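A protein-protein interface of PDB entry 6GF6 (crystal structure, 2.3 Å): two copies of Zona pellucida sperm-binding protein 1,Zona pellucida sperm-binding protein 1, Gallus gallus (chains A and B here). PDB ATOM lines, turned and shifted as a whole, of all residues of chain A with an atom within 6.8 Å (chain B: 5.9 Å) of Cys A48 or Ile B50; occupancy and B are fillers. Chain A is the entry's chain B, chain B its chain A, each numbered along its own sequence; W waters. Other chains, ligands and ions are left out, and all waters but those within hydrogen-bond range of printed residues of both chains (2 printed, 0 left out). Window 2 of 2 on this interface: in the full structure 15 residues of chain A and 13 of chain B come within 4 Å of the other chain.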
ATOM      1  N   ALA A  46      24.186 -30.882  13.121  1.00  0.00           N
ATOM      2  CA  ALA A  46      24.684 -30.951  14.487  1.00  0.00           C
ATOM      3  C   ALA A  46      23.939 -29.937  15.344  1.00  0.00           C
ATOM      4  O   ALA A  46      23.668 -28.812  14.911  1.00  0.00           O
ATOM      5  CB  ALA A  46      26.192 -30.678  14.550  1.00  0.00           C
ATOM      6  N   ASN A  47      23.654 -30.337  16.584  1.00  0.00           N
ATOM      7  CA  ASN A  47      22.944 -29.477  17.530  1.00  0.00           C
ATOM      8  C   ASN A  47      23.695 -28.176  17.778  1.00  0.00           C
ATOM      9  O   ASN A  47      23.124 -27.079  17.687  1.00  0.00           O
ATOM     10  CB  ASN A  47      22.766 -30.229  18.844  1.00  0.00           C
ATOM     11  CG  ASN A  47      21.653 -31.248  18.800  1.00  0.00           C
ATOM     12  OD1 ASN A  47      20.799 -31.255  17.902  1.00  0.00           O
ATOM     13  ND2 ASN A  47      21.705 -32.167  19.763  1.00  0.00           N
ATOM     14  N   CYS A  48      24.972 -28.283  18.140  1.00  0.00           N
ATOM     15  CA  CYS A  48      25.785 -27.119  18.476  1.00  0.00           C
ATOM     16  C   CYS A  48      26.218 -26.486  17.161  1.00  0.00           C
ATOM     17  O   CYS A  48      27.178 -26.926  16.521  1.00  0.00           O
ATOM     18  CB  CYS A  48      26.967 -27.524  19.348  1.00  0.00           C
ATOM     19  SG  CYS A  48      28.011 -26.150  19.849  1.00  0.00           S
ATOM     20  N   SER A  49      25.503 -25.451  16.747  1.00  0.00           N
ATOM     21  CA  SER A  49      25.673 -24.938  15.401  1.00  0.00           C
ATOM     22  C   SER A  49      25.018 -23.575  15.321  1.00  0.00           C
ATOM     23  O   SER A  49      24.073 -23.284  16.057  1.00  0.00           O
ATOM     24  CB  SER A  49      25.051 -25.899  14.371  1.00  0.00           C
ATOM     25  OG  SER A  49      25.100 -25.368  13.058  1.00  0.00           O
ATOM     26  N   ILE A  50      25.589 -22.722  14.473  1.00  0.00           N
ATOM     27  CA  ILE A  50      25.018 -21.410  14.202  1.00  0.00           C
ATOM     28  C   ILE A  50      23.813 -21.506  13.269  1.00  0.00           C
ATOM     29  O   ILE A  50      23.054 -20.539  13.144  1.00  0.00           O
ATOM     30  CB  ILE A  50      26.094 -20.481  13.608  1.00  0.00           C
ATOM     31  CG1 ILE A  50      25.659 -19.016  13.665  1.00  0.00           C
ATOM     32  CG2 ILE A  50      26.409 -20.871  12.176  1.00  0.00           C
ATOM     33  CD1 ILE A  50      25.692 -18.434  15.070  1.00  0.00           C
ATOM     34  N   CYS A  51      23.627 -22.645  12.603  1.00  0.00           N
ATOM     35  CA  CYS A  51      22.638 -22.780  11.543  1.00  0.00           C
ATOM     36  C   CYS A  51      21.208 -22.959  12.039  1.00  0.00           C
ATOM     37  O   CYS A  51      20.302 -23.064  11.208  1.00  0.00           O
ATOM     38  CB  CYS A  51      23.009 -23.974  10.654  1.00  0.00           C
ATOM     39  SG  CYS A  51      24.377 -23.617   9.529  1.00  0.00           S
ATOM     40  N   MET A  52      20.997 -23.006  13.355  1.00  0.00           N
ATOM     41  CA  MET A  52      19.663 -23.086  13.952  1.00  0.00           C
ATOM     42  C   MET A  52      18.887 -24.293  13.426  1.00  0.00           C
ATOM     43  O   MET A  52      17.753 -24.178  12.954  1.00  0.00           O
ATOM     44  CB  MET A  52      18.887 -21.785  13.730  1.00  0.00           C
ATOM     45  CG  MET A  52      19.618 -20.546  14.223  1.00  0.00           C
ATOM     46  SD  MET A  52      20.086 -20.649  15.963  1.00  0.00           S
ATOM     47  CE  MET A  52      21.101 -19.182  16.137  1.00  0.00           C
ATOM     48  N   HIS A  53      19.513 -25.465  13.511  1.00  0.00           N
ATOM     49  CA  HIS A  53      18.852 -26.719  13.181  1.00  0.00           C
ATOM     50  C   HIS A  53      19.280 -27.786  14.177  1.00  0.00           C
ATOM     51  O   HIS A  53      20.390 -27.747  14.714  1.00  0.00           O
ATOM     52  CB  HIS A  53      19.121 -27.173  11.732  1.00  0.00           C
ATOM     53  CG  HIS A  53      20.572 -27.273  11.370  1.00  0.00           C
ATOM     54  ND1 HIS A  53      21.020 -27.111  10.076  1.00  0.00           N
ATOM     55  CD2 HIS A  53      21.669 -27.539  12.116  1.00  0.00           C
ATOM     56  CE1 HIS A  53      22.332 -27.262  10.045  1.00  0.00           C
ATOM     57  NE2 HIS A  53      22.751 -27.521  11.270  1.00  0.00           N
ATOM     58  N   TRP A  54      18.377 -28.731  14.437  1.00  0.00           N
ATOM     59  CA  TRP A  54      18.582 -29.683  15.517  1.00  0.00           C
ATOM     60  C   TRP A  54      17.980 -31.033  15.154  1.00  0.00           C
ATOM     61  O   TRP A  54      17.143 -31.150  14.255  1.00  0.00           O
ATOM     62  CB  TRP A  54      17.972 -29.177  16.833  1.00  0.00           C
ATOM     63  CG  TRP A  54      18.441 -27.813  17.242  1.00  0.00           C
ATOM     64  CD1 TRP A  54      19.500 -27.517  18.050  1.00  0.00           C
ATOM     65  CD2 TRP A  54      17.865 -26.558  16.860  1.00  0.00           C
ATOM     66  NE1 TRP A  54      19.620 -26.156  18.195  1.00  0.00           N
ATOM     67  CE2 TRP A  54      18.628 -25.543  17.472  1.00  0.00           C
ATOM     68  CE3 TRP A  54      16.779 -26.192  16.058  1.00  0.00           C
ATOM     69  CZ2 TRP A  54      18.339 -24.189  17.311  1.00  0.00           C
ATOM     70  CZ3 TRP A  54      16.493 -24.847  15.898  1.00  0.00           C
ATOM     71  CH2 TRP A  54      17.270 -23.862  16.522  1.00  0.00           C
ATOM     72  N   ASN B  47      27.022 -27.046  27.140  1.00  0.00           N
ATOM     73  CA  ASN B  47      27.923 -25.989  26.714  1.00  0.00           C
ATOM     74  C   ASN B  47      28.072 -26.005  25.206  1.00  0.00           C
ATOM     75  O   ASN B  47      28.419 -27.030  24.613  1.00  0.00           O
ATOM     76  CB  ASN B  47      29.304 -26.132  27.350  1.00  0.00           C
ATOM     77  CG  ASN B  47      29.378 -25.550  28.734  1.00  0.00           C
ATOM     78  OD1 ASN B  47      28.408 -24.989  29.247  1.00  0.00           O
ATOM     79  ND2 ASN B  47      30.564 -25.622  29.325  1.00  0.00           N
ATOM     80  N   CYS B  48      27.798 -24.859  24.595  1.00  0.00           N
ATOM     81  CA  CYS B  48      27.879 -24.694  23.149  1.00  0.00           C
ATOM     82  C   CYS B  48      28.098 -23.210  22.899  1.00  0.00           C
ATOM     83  O   CYS B  48      27.140 -22.430  22.894  1.00  0.00           O
ATOM     84  CB  CYS B  48      26.631 -25.186  22.434  1.00  0.00           C
ATOM     85  SG  CYS B  48      26.683 -24.833  20.654  1.00  0.00           S
ATOM     86  N   SER B  49      29.356 -22.839  22.690  1.00  0.00           N
ATOM     87  CA  SER B  49      29.700 -21.429  22.604  1.00  0.00           C
ATOM     88  C   SER B  49      29.049 -20.764  21.392  1.00  0.00           C
ATOM     89  O   SER B  49      28.556 -19.637  21.495  1.00  0.00           O
ATOM     90  CB  SER B  49      31.218 -21.280  22.562  1.00  0.00           C
ATOM     91  OG  SER B  49      31.586 -19.923  22.411  1.00  0.00           O
ATOM     92  N   ILE B  50      28.963 -21.464  20.254  1.00  0.00           N
ATOM     93  CA  ILE B  50      28.378 -20.829  19.076  1.00  0.00           C
ATOM     94  C   ILE B  50      26.879 -20.608  19.256  1.00  0.00           C
ATOM     95  O   ILE B  50      26.312 -19.713  18.619  1.00  0.00           O
ATOM     96  CB  ILE B  50      28.679 -21.666  17.812  1.00  0.00           C
ATOM     97  CG1 ILE B  50      28.382 -20.867  16.541  1.00  0.00           C
ATOM     98  CG2 ILE B  50      27.890 -22.978  17.800  1.00  0.00           C
ATOM     99  CD1 ILE B  50      29.383 -19.772  16.259  1.00  0.00           C
ATOM    100  N   CYS B  51      26.226 -21.393  20.122  1.00  0.00           N
ATOM    101  CA  CYS B  51      24.827 -21.189  20.486  1.00  0.00           C
ATOM    102  C   CYS B  51      24.659 -20.175  21.608  1.00  0.00           C
ATOM    103  O   CYS B  51      23.525 -19.788  21.904  1.00  0.00           O
ATOM    104  CB  CYS B  51      24.164 -22.502  20.928  1.00  0.00           C
ATOM    105  SG  CYS B  51      23.505 -23.539  19.612  1.00  0.00           S
ATOM    106  N   MET B  52      25.748 -19.773  22.257  1.00  0.00           N
ATOM    107  CA  MET B  52      25.691 -18.889  23.422  1.00  0.00           C
ATOM    108  C   MET B  52      24.928 -19.549  24.567  1.00  0.00           C
ATOM    109  O   MET B  52      24.099 -18.924  25.232  1.00  0.00           O
ATOM    110  CB  MET B  52      25.079 -17.533  23.067  1.00  0.00           C
ATOM    111  CG  MET B  52      25.800 -16.824  21.922  1.00  0.00           C
ATOM    112  SD  MET B  52      25.276 -15.112  21.729  1.00  0.00           S
ATOM    113  CE  MET B  52      25.507 -14.897  19.967  1.00  0.00           C
ATOM    114  N   HIS B  53      25.206 -20.826  24.797  1.00  0.00           N
ATOM    115  CA  HIS B  53      24.681 -21.544  25.946  1.00  0.00           C
ATOM    116  C   HIS B  53      25.834 -22.019  26.816  1.00  0.00           C
ATOM    117  O   HIS B  53      26.794 -22.614  26.317  1.00  0.00           O
ATOM    118  CB  HIS B  53      23.869 -22.780  25.519  1.00  0.00           C
ATOM    119  CG  HIS B  53      22.588 -22.470  24.813  1.00  0.00           C
ATOM    120  ND1 HIS B  53      21.714 -23.455  24.408  1.00  0.00           N
ATOM    121  CD2 HIS B  53      22.031 -21.297  24.437  1.00  0.00           C
ATOM    122  CE1 HIS B  53      20.674 -22.901  23.809  1.00  0.00           C
ATOM    123  NE2 HIS B  53      20.840 -21.591  23.817  1.00  0.00           N
ATOM    124  N   GLU B  70      21.222 -13.518  21.615  1.00  0.00           N
ATOM    125  CA  GLU B  70      21.285 -13.921  20.219  1.00  0.00           C
ATOM    126  C   GLU B  70      21.663 -15.394  20.058  1.00  0.00           C
ATOM    127  O   GLU B  70      22.202 -15.777  19.015  1.00  0.00           O
ATOM    128  CB  GLU B  70      22.240 -12.999  19.454  1.00  0.00           C
ATOM    129  CG  GLU B  70      21.806 -11.527  19.531  1.00  0.00           C
ATOM    130  CD  GLU B  70      22.771 -10.556  18.865  1.00  0.00           C
ATOM    131  OE1 GLU B  70      24.000 -10.682  19.059  1.00  0.00           O
ATOM    132  OE2 GLU B  70      22.287  -9.654  18.149  1.00  0.00           O
ATOM    133  N   GLY B  71      21.440 -16.215  21.090  1.00  0.00           N
ATOM    134  CA  GLY B  71      21.796 -17.617  21.047  1.00  0.00           C
ATOM    135  C   GLY B  71      20.670 -18.507  20.538  1.00  0.00           C
ATOM    136  O   GLY B  71      19.558 -18.065  20.260  1.00  0.00           O
ATOM    137  N   CYS B  72      20.953 -19.809  20.519  1.00  0.00           N
ATOM    138  CA  CYS B  72      20.032 -20.771  19.922  1.00  0.00           C
ATOM    139  C   CYS B  72      18.697 -20.779  20.669  1.00  0.00           C
ATOM    140  O   CYS B  72      18.652 -20.806  21.904  1.00  0.00           O
ATOM    141  CB  CYS B  72      20.679 -22.169  19.909  1.00  0.00           C
ATOM    142  SG  CYS B  72      22.128 -22.297  18.751  1.00  0.00           S
HETATM  143  O   HOH W   1      21.087 -25.636  20.466  1.00  0.00           O
HETATM  144  O   HOH W   2      30.587 -23.950  19.712  1.00  0.00           O
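SG of Cys A48 is disulfide-bonded to SG of Cys B48 (2.0 Å).
The backbone carbonyl oxygen (O) of Ser A49 lies close to the side-chain sulfur (SG) of Cys B51 (3.6 Å).
O of Ser A49 lies close to SG of Cys B72 (3.5 Å).
The side-chain sulfur of Cys B48 lies close to the backbone NH of Cys B51, 3.5 Å away.
SG of Cys B51 is disulfide-bonded to SG of Cys B72 (2.0 Å).
A ring nitrogen (NE2) of His B53 sits at hydrogen-bond distance from the backbone carbonyl oxygen (O) of Cys B72, 3.0 Å away.
The backbone NH (N) of Cys B48 lies within hydrogen-bond range of the backbone carbonyl oxygen (O) of His B53 (3.0 Å).
The side-chain hydroxyl (OG) of Ser A49 is in hydrogen-bond range of the backbone NH (N) of Cys A51, at 3.1 Å.
SG of Cys A48 touches CG2 of Ile B50, 3.8 Å away.
Ser A49 touches Ile B50 (N to CG2, 3.6 Å).
Ile A50 touches Ile B50.
Cys B72 touches Met A52 (SG to SD, 3.8 Å).
Cys A48 touches two residues of chain B.
Of the printed residues of chain B, Ser A49 touches Ile B50 (3.6 Å), Cys B51 (3.6 Å) and Cys B72 (3.5 Å).
Of the printed residues of chain B, Ile A50 touches Ile B50 (3.7 Å).
Printed residues of chain B within 4 Å of Met A52: Cys B72 (3.8 Å).
Asn B47 touches none of the printed residues of chain A.
Of the printed residues of chain A, Cys B48 touches Cys A48 (2.0 Å).
Of chain A, only Cys A48, Ser A49 and Ile A50 come within 4 Å of Ile B50.
Printed residues of chain A within 4 Å of Cys B51: Ser A49 (3.6 Å).
His B53 touches none of the printed residues of chain A.
The nearest residue of chain B that does not touch Cys A48 is Cys B51 (4.4 Å).
The nearest printed residue of chain A that does not touch Ile B50 is Met A52 (5.8 Å).
The nearest printed residue of chain A that does not touch Cys B48 is Ser A49 (4.1 Å).
Hydrophobic or aromatic side chains of chain B that line the printed part of chain A: Ile B50.
Along chain B the printed residues that touch a printed residue of chain A span positions 48 to 72.
Printed residues of chain A that touch a printed residue of chain B: Cys A48, Ser A49, Ile A50 and Met A52.
Hydrophobic or aromatic side chains of chain A that line the printed part of chain B: Ile A50 and Met A52.
Along chain A the printed residues that touch a printed residue of chain B span positions 48 to 52.
Among the printed residues, 7 pairs touch across the chains.
Cys B48 touches its own counterpart, Cys A48.
Cys A48 touches Ile B50, but with the chains exchanged Ile A50 does not touch Cys B48 (6.6 Å).
Ser A49 touches Ile B50, but with the chains exchanged Ile A50 does not touch Ser B49 (7.1 Å).
Ile A50 touches its own counterpart, Ile B50.
Positions printed for both chains: 47, 48, 49, 50, 51, 52 and 53.
Of the 7 pairs that touch across the chains among the printed residues, 2 have their exchanged pair printed and touching as well.
Water W1 bridges NE1 of Trp A54 (2.8 Å) and SG of Cys B51 (3.3 Å).
Water W2 lies within hydrogen-bond range of N of Ile B50, SG of Cys A48 and N of Ser B49.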
